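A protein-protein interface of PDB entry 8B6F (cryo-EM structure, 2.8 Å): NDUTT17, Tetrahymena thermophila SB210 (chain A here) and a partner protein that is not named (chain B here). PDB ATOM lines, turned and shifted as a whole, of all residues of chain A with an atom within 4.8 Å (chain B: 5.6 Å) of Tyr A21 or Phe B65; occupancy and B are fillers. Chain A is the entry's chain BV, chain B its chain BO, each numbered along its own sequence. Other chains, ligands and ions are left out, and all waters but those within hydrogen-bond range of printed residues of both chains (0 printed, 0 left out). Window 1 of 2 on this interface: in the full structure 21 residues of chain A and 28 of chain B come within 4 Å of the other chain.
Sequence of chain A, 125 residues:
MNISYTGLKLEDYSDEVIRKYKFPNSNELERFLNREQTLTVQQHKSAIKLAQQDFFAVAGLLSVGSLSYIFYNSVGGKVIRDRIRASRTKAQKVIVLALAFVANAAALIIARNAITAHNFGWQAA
NZ of Lys B69 lies within salt-bridge range of OE1 of Glu B89.
The side-chain amino group of Lys B69 lies within salt-bridge range of the side-chain carboxylate of Asp B73 (2.9 Å).
The side-chain carboxylate (OD1) of Asp B73 sits close to the backbone NH (N) of Ile B88 (3.3 Å).
Of the printed residues of chain B, Tyr A21 touches Gly B64 (2.4 Å), Phe B65 (3.4 Å), Leu B66 (3.5 Å), Lys B69 (3.7 Å), Val B72 (3.8 Å), Ile B88 (3.9 Å), Glu B89 (3.98 Å), Phe B103 (3.3 Å) and Phe B107 (3.8 Å).
Of the printed residues of chain B, Lys A22 touches Gln B108.
Phe B65 touches just these residues of chain A: Tyr A21, Phe A23 and Pro A24.
Of the printed residues of chain A, Val B72 touches Tyr A21.
Of the printed residues of chain A, Gln B108 touches Lys A20, Lys A22 and Pro A24.
Hydrophobic or aromatic side chains of chain B that line the printed part of chain A: Met B49, Leu B63, Phe B65, Leu B66, Pro B67, Val B72, Ile B88, Phe B103, Phe B107 and Leu B110.
Hydrophobic or aromatic side chains of chain A within 4 Å of the printed part of chain B: Tyr A5, Val A17, Tyr A21, Phe A23 and Pro A24.
Among the printed residues, Asp or Glu carboxylates within 4 Å of a Lys or Arg side-chain nitrogen of the other chain: Lys A20 with Glu B89.
Among the printed residues, pairs that only touch across the chains: Tyr A5 with Leu B63 (3.1 Å), Tyr A21 with Phe B103 (3.3 Å), Phe A23 with Gly B64 (3.3 Å), Pro A24 with Gln B108 (3.3 Å), Pro A24 with Phe B107 (3.4 Å), Tyr A21 with Phe B65 (3.4 Å), Tyr A21 with Leu B66 (3.5 Å), Lys A20 with Phe B103 (3.5 Å), Pro A24 with Leu B110 (3.6 Å), Val A17 with Lys B69 (3.6 Å), Val A17 with Glu B89 (3.7 Å), Tyr A21 with Lys B69 (3.7 Å), Phe A23 with Phe B65 (3.7 Å), Tyr A21 with Phe B107 (3.8 Å), Tyr A21 with Val B72 (3.8 Å), Tyr A21 with Ile B88 (3.9 Å), Phe A23 with Met B49 (3.9 Å), Pro A24 with Phe B65 (3.9 Å), Tyr A21 with Glu B89 (3.98 Å) and Tyr A5 with Pro B67 (3.98 Å).
The side-chain carboxylate (OE2) of Glu B89 lies within salt-bridge range of the side-chain amino group (NZ) of Lys A20 (2.7 Å).
The side-chain amide nitrogen (NE2) of Gln B108 sits at hydrogen-bond distance from the backbone carbonyl oxygen (O) of Lys A22 (2.8 Å).
SD of Met B49 lies close to OH of Tyr A5.
The backbone carbonyl oxygen (O) of Tyr A21 sits close to the backbone carbonyl oxygen (O) of Gly B64 (2.4 Å).
The backbone carbonyl oxygen (O) of Lys A20 lies close to the side-chain amide oxygen (OE1) of Gln B108 (3.4 Å).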
ATOM      1  N   TYR A   5       9.582 -14.637 -15.029  1.00  0.00           N
ATOM      2  CA  TYR A   5      10.860 -13.940 -15.054  1.00  0.00           C
ATOM      3  C   TYR A   5      10.716 -12.429 -14.935  1.00  0.00           C
ATOM      4  O   TYR A   5      11.724 -11.746 -14.723  1.00  0.00           O
ATOM      5  CB  TYR A   5      11.614 -14.272 -16.341  1.00  0.00           C
ATOM      6  CG  TYR A   5      12.091 -15.702 -16.430  1.00  0.00           C
ATOM      7  CD1 TYR A   5      13.282 -16.095 -15.837  1.00  0.00           C
ATOM      8  CD2 TYR A   5      11.357 -16.655 -17.120  1.00  0.00           C
ATOM      9  CE1 TYR A   5      13.726 -17.399 -15.921  1.00  0.00           C
ATOM     10  CE2 TYR A   5      11.792 -17.963 -17.209  1.00  0.00           C
ATOM     11  CZ  TYR A   5      12.978 -18.327 -16.609  1.00  0.00           C
ATOM     12  OH  TYR A   5      13.416 -19.626 -16.694  1.00  0.00           O
ATOM     13  N   VAL A  17      23.681 -17.795  -4.883  1.00  0.00           N
ATOM     14  CA  VAL A  17      22.296 -18.113  -5.214  1.00  0.00           C
ATOM     15  C   VAL A  17      22.135 -18.284  -6.719  1.00  0.00           C
ATOM     16  O   VAL A  17      21.432 -19.189  -7.182  1.00  0.00           O
ATOM     17  CB  VAL A  17      21.354 -17.029  -4.659  1.00  0.00           C
ATOM     18  CG1 VAL A  17      19.915 -17.285  -5.090  1.00  0.00           C
ATOM     19  CG2 VAL A  17      21.451 -16.969  -3.147  1.00  0.00           C
ATOM     20  N   ILE A  18      22.784 -17.423  -7.505  1.00  0.00           N
ATOM     21  CA  ILE A  18      22.708 -17.548  -8.959  1.00  0.00           C
ATOM     22  C   ILE A  18      23.347 -18.854  -9.410  1.00  0.00           C
ATOM     23  O   ILE A  18      22.794 -19.584 -10.239  1.00  0.00           O
ATOM     24  CB  ILE A  18      23.368 -16.333  -9.636  1.00  0.00           C
ATOM     25  CG1 ILE A  18      22.597 -15.055  -9.302  1.00  0.00           C
ATOM     26  CG2 ILE A  18      23.435 -16.529 -11.147  1.00  0.00           C
ATOM     27  CD1 ILE A  18      23.351 -13.784  -9.635  1.00  0.00           C
ATOM     28  N   ARG A  19      24.526 -19.167  -8.869  1.00  0.00           N
ATOM     29  CA  ARG A  19      25.187 -20.419  -9.217  1.00  0.00           C
ATOM     30  C   ARG A  19      24.301 -21.606  -8.869  1.00  0.00           C
ATOM     31  O   ARG A  19      24.233 -22.586  -9.619  1.00  0.00           O
ATOM     32  CB  ARG A  19      26.534 -20.511  -8.498  1.00  0.00           C
ATOM     33  CG  ARG A  19      27.431 -21.665  -8.950  1.00  0.00           C
ATOM     34  CD  ARG A  19      27.118 -22.975  -8.232  1.00  0.00           C
ATOM     35  NE  ARG A  19      27.146 -22.833  -6.781  1.00  0.00           N
ATOM     36  CZ  ARG A  19      26.756 -23.771  -5.927  1.00  0.00           C
ATOM     37  NH1 ARG A  19      26.299 -24.940  -6.345  1.00  0.00           N
ATOM     38  NH2 ARG A  19      26.825 -23.529  -4.622  1.00  0.00           N
ATOM     39  N   LYS A  20      23.610 -21.532  -7.733  1.00  0.00           N
ATOM     40  CA  LYS A  20      22.701 -22.599  -7.336  1.00  0.00           C
ATOM     41  C   LYS A  20      21.535 -22.716  -8.309  1.00  0.00           C
ATOM     42  O   LYS A  20      21.225 -23.810  -8.795  1.00  0.00           O
ATOM     43  CB  LYS A  20      22.202 -22.337  -5.916  1.00  0.00           C
ATOM     44  CG  LYS A  20      21.881 -23.583  -5.126  1.00  0.00           C
ATOM     45  CD  LYS A  20      21.960 -23.309  -3.634  1.00  0.00           C
ATOM     46  CE  LYS A  20      20.990 -22.218  -3.210  1.00  0.00           C
ATOM     47  NZ  LYS A  20      21.025 -21.996  -1.739  1.00  0.00           N
ATOM     48  N   TYR A  21      20.875 -21.601  -8.601  1.00  0.00           N
ATOM     49  CA  TYR A  21      19.797 -21.557  -9.589  1.00  0.00           C
ATOM     50  C   TYR A  21      20.325 -21.174 -10.968  1.00  0.00           C
ATOM     51  O   TYR A  21      19.827 -20.248 -11.601  1.00  0.00           O
ATOM     52  CB  TYR A  21      18.717 -20.581  -9.137  1.00  0.00           C
ATOM     53  CG  TYR A  21      18.101 -20.895  -7.795  1.00  0.00           C
ATOM     54  CD1 TYR A  21      17.045 -21.787  -7.687  1.00  0.00           C
ATOM     55  CD2 TYR A  21      18.565 -20.286  -6.638  1.00  0.00           C
ATOM     56  CE1 TYR A  21      16.473 -22.072  -6.463  1.00  0.00           C
ATOM     57  CE2 TYR A  21      18.000 -20.564  -5.409  1.00  0.00           C
ATOM     58  CZ  TYR A  21      16.955 -21.456  -5.329  1.00  0.00           C
ATOM     59  OH  TYR A  21      16.390 -21.737  -4.108  1.00  0.00           O
ATOM     60  N   LYS A  22      21.359 -21.864 -11.436  1.00  0.00           N
ATOM     61  CA  LYS A  22      21.848 -21.702 -12.796  1.00  0.00           C
ATOM     62  C   LYS A  22      21.380 -22.859 -13.671  1.00  0.00           C
ATOM     63  O   LYS A  22      21.255 -23.996 -13.215  1.00  0.00           O
ATOM     64  CB  LYS A  22      23.377 -21.617 -12.820  1.00  0.00           C
ATOM     65  CG  LYS A  22      24.079 -22.954 -12.625  1.00  0.00           C
ATOM     66  CD  LYS A  22      25.580 -22.769 -12.464  1.00  0.00           C
ATOM     67  CE  LYS A  22      26.277 -24.098 -12.245  1.00  0.00           C
ATOM     68  NZ  LYS A  22      26.054 -25.040 -13.378  1.00  0.00           N
ATOM     69  N   PHE A  23      21.116 -22.550 -14.936  1.00  0.00           N
ATOM     70  CA  PHE A  23      20.695 -23.580 -15.871  1.00  0.00           C
ATOM     71  C   PHE A  23      21.819 -24.595 -16.066  1.00  0.00           C
ATOM     72  O   PHE A  23      22.993 -24.215 -16.139  1.00  0.00           O
ATOM     73  CB  PHE A  23      20.324 -22.960 -17.221  1.00  0.00           C
ATOM     74  CG  PHE A  23      18.866 -22.614 -17.365  1.00  0.00           C
ATOM     75  CD1 PHE A  23      17.877 -23.504 -16.979  1.00  0.00           C
ATOM     76  CD2 PHE A  23      18.488 -21.399 -17.908  1.00  0.00           C
ATOM     77  CE1 PHE A  23      16.541 -23.183 -17.123  1.00  0.00           C
ATOM     78  CE2 PHE A  23      17.154 -21.074 -18.053  1.00  0.00           C
ATOM     79  CZ  PHE A  23      16.181 -21.968 -17.660  1.00  0.00           C
ATOM     80  N   PRO A  24      21.504 -25.888 -16.158  1.00  0.00           N
ATOM     81  CA  PRO A  24      22.551 -26.877 -16.448  1.00  0.00           C
ATOM     82  C   PRO A  24      22.990 -26.850 -17.902  1.00  0.00           C
ATOM     83  O   PRO A  24      22.569 -25.981 -18.673  1.00  0.00           O
ATOM     84  CB  PRO A  24      21.883 -28.208 -16.080  1.00  0.00           C
ATOM     85  CG  PRO A  24      20.439 -27.967 -16.284  1.00  0.00           C
ATOM     86  CD  PRO A  24      20.196 -26.527 -15.924  1.00  0.00           C
ATOM     87  N   CYS B  45       6.924 -25.841 -11.899  1.00  0.00           N
ATOM     88  CA  CYS B  45       7.651 -24.622 -12.230  1.00  0.00           C
ATOM     89  C   CYS B  45       9.010 -24.927 -12.843  1.00  0.00           C
ATOM     90  O   CYS B  45       9.465 -24.191 -13.724  1.00  0.00           O
ATOM     91  CB  CYS B  45       7.818 -23.754 -10.983  1.00  0.00           C
ATOM     92  SG  CYS B  45       8.569 -22.146 -11.308  1.00  0.00           S
ATOM     93  N   ARG B  46       9.670 -26.000 -12.406  1.00  0.00           N
ATOM     94  CA  ARG B  46      10.919 -26.395 -13.047  1.00  0.00           C
ATOM     95  C   ARG B  46      10.696 -26.711 -14.520  1.00  0.00           C
ATOM     96  O   ARG B  46      11.434 -26.234 -15.389  1.00  0.00           O
ATOM     97  CB  ARG B  46      11.525 -27.595 -12.317  1.00  0.00           C
ATOM     98  CG  ARG B  46      12.858 -28.054 -12.888  1.00  0.00           C
ATOM     99  CD  ARG B  46      13.421 -29.238 -12.125  1.00  0.00           C
ATOM    100  NE  ARG B  46      12.584 -30.424 -12.253  1.00  0.00           N
ATOM    101  CZ  ARG B  46      12.931 -31.636 -11.843  1.00  0.00           C
ATOM    102  NH1 ARG B  46      14.103 -31.864 -11.276  1.00  0.00           N
ATOM    103  NH2 ARG B  46      12.081 -32.644 -12.008  1.00  0.00           N
ATOM    104  N   MET B  49       9.884 -23.413 -16.439  1.00  0.00           N
ATOM    105  CA  MET B  49      11.049 -22.572 -16.693  1.00  0.00           C
ATOM    106  C   MET B  49      11.943 -23.172 -17.771  1.00  0.00           C
ATOM    107  O   MET B  49      12.459 -22.446 -18.627  1.00  0.00           O
ATOM    108  CB  MET B  49      11.841 -22.366 -15.402  1.00  0.00           C
ATOM    109  CG  MET B  49      11.103 -21.591 -14.316  1.00  0.00           C
ATOM    110  SD  MET B  49      10.514 -19.974 -14.847  1.00  0.00           S
ATOM    111  CE  MET B  49       8.830 -20.353 -15.324  1.00  0.00           C
ATOM    112  N   VAL B  50      12.143 -24.490 -17.749  1.00  0.00           N
ATOM    113  CA  VAL B  50      12.958 -25.121 -18.784  1.00  0.00           C
ATOM    114  C   VAL B  50      12.329 -24.910 -20.155  1.00  0.00           C
ATOM    115  O   VAL B  50      13.025 -24.608 -21.132  1.00  0.00           O
ATOM    116  CB  VAL B  50      13.155 -26.617 -18.474  1.00  0.00           C
ATOM    117  CG1 VAL B  50      13.798 -27.334 -19.655  1.00  0.00           C
ATOM    118  CG2 VAL B  50      14.004 -26.790 -17.226  1.00  0.00           C
ATOM    119  N   LEU B  63      18.499 -16.090 -16.278  1.00  0.00           N
ATOM    120  CA  LEU B  63      17.743 -16.050 -15.032  1.00  0.00           C
ATOM    121  C   LEU B  63      17.139 -17.406 -14.684  1.00  0.00           C
ATOM    122  O   LEU B  63      16.146 -17.466 -13.956  1.00  0.00           O
ATOM    123  CB  LEU B  63      16.640 -14.995 -15.120  1.00  0.00           C
ATOM    124  CG  LEU B  63      17.078 -13.571 -15.470  1.00  0.00           C
ATOM    125  CD1 LEU B  63      15.870 -12.668 -15.642  1.00  0.00           C
ATOM    126  CD2 LEU B  63      18.008 -13.020 -14.409  1.00  0.00           C
ATOM    127  N   GLY B  64      17.723 -18.492 -15.180  1.00  0.00           N
ATOM    128  CA  GLY B  64      17.124 -19.805 -15.050  1.00  0.00           C
ATOM    129  C   GLY B  64      16.816 -20.219 -13.627  1.00  0.00           C
ATOM    130  O   GLY B  64      17.667 -20.108 -12.743  1.00  0.00           O
ATOM    131  N   PHE B  65      15.594 -20.692 -13.396  1.00  0.00           N
ATOM    132  CA  PHE B  65      15.139 -21.281 -12.140  1.00  0.00           C
ATOM    133  C   PHE B  65      15.055 -20.278 -10.996  1.00  0.00           C
ATOM    134  O   PHE B  65      14.696 -20.672  -9.882  1.00  0.00           O
ATOM    135  CB  PHE B  65      16.026 -22.454 -11.699  1.00  0.00           C
ATOM    136  CG  PHE B  65      15.985 -23.632 -12.633  1.00  0.00           C
ATOM    137  CD1 PHE B  65      14.782 -24.076 -13.160  1.00  0.00           C
ATOM    138  CD2 PHE B  65      17.149 -24.288 -12.990  1.00  0.00           C
ATOM    139  CE1 PHE B  65      14.744 -25.154 -14.019  1.00  0.00           C
ATOM    140  CE2 PHE B  65      17.117 -25.367 -13.849  1.00  0.00           C
ATOM    141  CZ  PHE B  65      15.912 -25.800 -14.364  1.00  0.00           C
ATOM    142  N   LEU B  66      15.374 -19.007 -11.219  1.00  0.00           N
ATOM    143  CA  LEU B  66      15.159 -18.015 -10.171  1.00  0.00           C
ATOM    144  C   LEU B  66      13.705 -17.961  -9.724  1.00  0.00           C
ATOM    145  O   LEU B  66      13.466 -17.857  -8.508  1.00  0.00           O
ATOM    146  CB  LEU B  66      15.640 -16.637 -10.642  1.00  0.00           C
ATOM    147  CG  LEU B  66      17.116 -16.337 -10.360  1.00  0.00           C
ATOM    148  CD1 LEU B  66      18.019 -17.360 -11.023  1.00  0.00           C
ATOM    149  CD2 LEU B  66      17.476 -14.935 -10.817  1.00  0.00           C
ATOM    150  N   PRO B  67      12.710 -18.010 -10.613  1.00  0.00           N
ATOM    151  CA  PRO B  67      11.318 -18.051 -10.140  1.00  0.00           C
ATOM    152  C   PRO B  67      11.025 -19.223  -9.220  1.00  0.00           C
ATOM    153  O   PRO B  67      10.144 -19.114  -8.360  1.00  0.00           O
ATOM    154  CB  PRO B  67      10.515 -18.134 -11.445  1.00  0.00           C
ATOM    155  CG  PRO B  67      11.389 -17.477 -12.453  1.00  0.00           C
ATOM    156  CD  PRO B  67      12.789 -17.856 -12.076  1.00  0.00           C
ATOM    157  N   CYS B  68      11.728 -20.346  -9.379  1.00  0.00           N
ATOM    158  CA  CYS B  68      11.574 -21.466  -8.460  1.00  0.00           C
ATOM    159  C   CYS B  68      12.108 -21.159  -7.068  1.00  0.00           C
ATOM    160  O   CYS B  68      11.826 -21.917  -6.136  1.00  0.00           O
ATOM    161  CB  CYS B  68      12.283 -22.707  -9.005  1.00  0.00           C
ATOM    162  SG  CYS B  68      11.625 -23.330 -10.562  1.00  0.00           S
ATOM    163  N   LYS B  69      12.860 -20.069  -6.904  1.00  0.00           N
ATOM    164  CA  LYS B  69      13.434 -19.758  -5.599  1.00  0.00           C
ATOM    165  C   LYS B  69      12.346 -19.500  -4.566  1.00  0.00           C
ATOM    166  O   LYS B  69      12.449 -19.949  -3.420  1.00  0.00           O
ATOM    167  CB  LYS B  69      14.366 -18.552  -5.709  1.00  0.00           C
ATOM    168  CG  LYS B  69      15.147 -18.262  -4.436  1.00  0.00           C
ATOM    169  CD  LYS B  69      15.981 -17.001  -4.572  1.00  0.00           C
ATOM    170  CE  LYS B  69      16.807 -16.745  -3.321  1.00  0.00           C
ATOM    171  NZ  LYS B  69      15.964 -16.605  -2.102  1.00  0.00           N
ATOM    172  N   VAL B  72      10.886 -22.824  -3.499  1.00  0.00           N
ATOM    173  CA  VAL B  72      11.799 -23.577  -2.644  1.00  0.00           C
ATOM    174  C   VAL B  72      11.826 -22.980  -1.244  1.00  0.00           C
ATOM    175  O   VAL B  72      11.802 -23.705  -0.244  1.00  0.00           O
ATOM    176  CB  VAL B  72      13.206 -23.623  -3.269  1.00  0.00           C
ATOM    177  CG1 VAL B  72      14.213 -24.222  -2.295  1.00  0.00           C
ATOM    178  CG2 VAL B  72      13.186 -24.421  -4.559  1.00  0.00           C
ATOM    179  N   ASP B  73      11.883 -21.651  -1.150  1.00  0.00           N
ATOM    180  CA  ASP B  73      11.900 -21.009   0.160  1.00  0.00           C
ATOM    181  C   ASP B  73      10.602 -21.261   0.912  1.00  0.00           C
ATOM    182  O   ASP B  73      10.615 -21.515   2.121  1.00  0.00           O
ATOM    183  CB  ASP B  73      12.144 -19.509   0.004  1.00  0.00           C
ATOM    184  CG  ASP B  73      13.484 -19.202  -0.626  1.00  0.00           C
ATOM    185  OD1 ASP B  73      14.396 -20.047  -0.524  1.00  0.00           O
ATOM    186  OD2 ASP B  73      13.631 -18.112  -1.215  1.00  0.00           O
ATOM    187  N   ILE B  88      16.017 -20.854   2.246  1.00  0.00           N
ATOM    188  CA  ILE B  88      16.842 -22.055   2.172  1.00  0.00           C
ATOM    189  C   ILE B  88      18.302 -21.716   2.436  1.00  0.00           C
ATOM    190  O   ILE B  88      19.036 -22.515   3.030  1.00  0.00           O
ATOM    191  CB  ILE B  88      16.650 -22.749   0.808  1.00  0.00           C
ATOM    192  CG1 ILE B  88      17.397 -24.086   0.760  1.00  0.00           C
ATOM    193  CG2 ILE B  88      17.118 -21.847  -0.324  1.00  0.00           C
ATOM    194  CD1 ILE B  88      16.924 -25.109   1.773  1.00  0.00           C
ATOM    195  N   GLU B  89      18.751 -20.537   1.998  1.00  0.00           N
ATOM    196  CA  GLU B  89      20.126 -20.123   2.250  1.00  0.00           C
ATOM    197  C   GLU B  89      20.433 -20.025   3.738  1.00  0.00           C
ATOM    198  O   GLU B  89      21.601 -20.133   4.126  1.00  0.00           O
ATOM    199  CB  GLU B  89      20.410 -18.779   1.577  1.00  0.00           C
ATOM    200  CG  GLU B  89      20.642 -18.866   0.075  1.00  0.00           C
ATOM    201  CD  GLU B  89      19.388 -19.213  -0.700  1.00  0.00           C
ATOM    202  OE1 GLU B  89      18.283 -18.930  -0.198  1.00  0.00           O
ATOM    203  OE2 GLU B  89      19.506 -19.775  -1.809  1.00  0.00           O
ATOM    204  N   PHE B 103      19.814 -29.396  -4.112  1.00  0.00           N
ATOM    205  CA  PHE B 103      19.894 -28.457  -5.227  1.00  0.00           C
ATOM    206  C   PHE B 103      20.567 -29.095  -6.432  1.00  0.00           C
ATOM    207  O   PHE B 103      20.139 -28.891  -7.573  1.00  0.00           O
ATOM    208  CB  PHE B 103      20.636 -27.193  -4.799  1.00  0.00           C
ATOM    209  CG  PHE B 103      19.766 -26.203  -4.091  1.00  0.00           C
ATOM    210  CD1 PHE B 103      18.844 -25.450  -4.797  1.00  0.00           C
ATOM    211  CD2 PHE B 103      19.858 -26.032  -2.723  1.00  0.00           C
ATOM    212  CE1 PHE B 103      18.038 -24.540  -4.154  1.00  0.00           C
ATOM    213  CE2 PHE B 103      19.052 -25.124  -2.074  1.00  0.00           C
ATOM    214  CZ  PHE B 103      18.141 -24.377  -2.791  1.00  0.00           C
ATOM    215  N   THR B 106      18.034 -31.382  -8.088  1.00  0.00           N
ATOM    216  CA  THR B 106      16.878 -30.781  -8.741  1.00  0.00           C
ATOM    217  C   THR B 106      17.274 -29.965  -9.966  1.00  0.00           C
ATOM    218  O   THR B 106      16.690 -30.131 -11.041  1.00  0.00           O
ATOM    219  CB  THR B 106      16.116 -29.904  -7.744  1.00  0.00           C
ATOM    220  OG1 THR B 106      15.799 -30.668  -6.576  1.00  0.00           O
ATOM    221  CG2 THR B 106      14.824 -29.382  -8.356  1.00  0.00           C
ATOM    222  N   PHE B 107      18.261 -29.081  -9.826  1.00  0.00           N
ATOM    223  CA  PHE B 107      18.510 -28.070 -10.845  1.00  0.00           C
ATOM    224  C   PHE B 107      19.695 -28.376 -11.748  1.00  0.00           C
ATOM    225  O   PHE B 107      19.689 -27.959 -12.910  1.00  0.00           O
ATOM    226  CB  PHE B 107      18.730 -26.708 -10.178  1.00  0.00           C
ATOM    227  CG  PHE B 107      17.560 -26.248  -9.361  1.00  0.00           C
ATOM    228  CD1 PHE B 107      16.435 -25.728  -9.972  1.00  0.00           C
ATOM    229  CD2 PHE B 107      17.585 -26.338  -7.980  1.00  0.00           C
ATOM    230  CE1 PHE B 107      15.354 -25.306  -9.224  1.00  0.00           C
ATOM    231  CE2 PHE B 107      16.509 -25.916  -7.225  1.00  0.00           C
ATOM    232  CZ  PHE B 107      15.392 -25.399  -7.849  1.00  0.00           C
ATOM    233  N   GLN B 108      20.711 -29.087 -11.260  1.00  0.00           N
ATOM    234  CA  GLN B 108      21.868 -29.395 -12.091  1.00  0.00           C
ATOM    235  C   GLN B 108      21.725 -30.743 -12.788  1.00  0.00           C
ATOM    236  O   GLN B 108      21.865 -30.831 -14.011  1.00  0.00           O
ATOM    237  CB  GLN B 108      23.149 -29.361 -11.253  1.00  0.00           C
ATOM    238  CG  GLN B 108      23.843 -28.007 -11.253  1.00  0.00           C
ATOM    239  CD  GLN B 108      22.933 -26.878 -10.807  1.00  0.00           C
ATOM    240  OE1 GLN B 108      22.497 -26.833  -9.657  1.00  0.00           O
ATOM    241  NE2 GLN B 108      22.639 -25.961 -11.722  1.00  0.00           N
ATOM    242  N   LEU B 110      18.905 -32.433 -12.797  1.00  0.00           N
ATOM    243  CA  LEU B 110      17.528 -32.521 -13.278  1.00  0.00           C
ATOM    244  C   LEU B 110      16.961 -33.920 -13.056  1.00  0.00           C
ATOM    245  O   LEU B 110      16.268 -34.479 -13.908  1.00  0.00           O
ATOM    246  CB  LEU B 110      17.442 -32.121 -14.749  1.00  0.00           C
ATOM    247  CG  LEU B 110      17.850 -30.678 -15.066  1.00  0.00           C
ATOM    248  CD1 LEU B 110      17.821 -30.422 -16.555  1.00  0.00           C
ATOM    249  CD2 LEU B 110      16.945 -29.688 -14.358  1.00  0.00           C
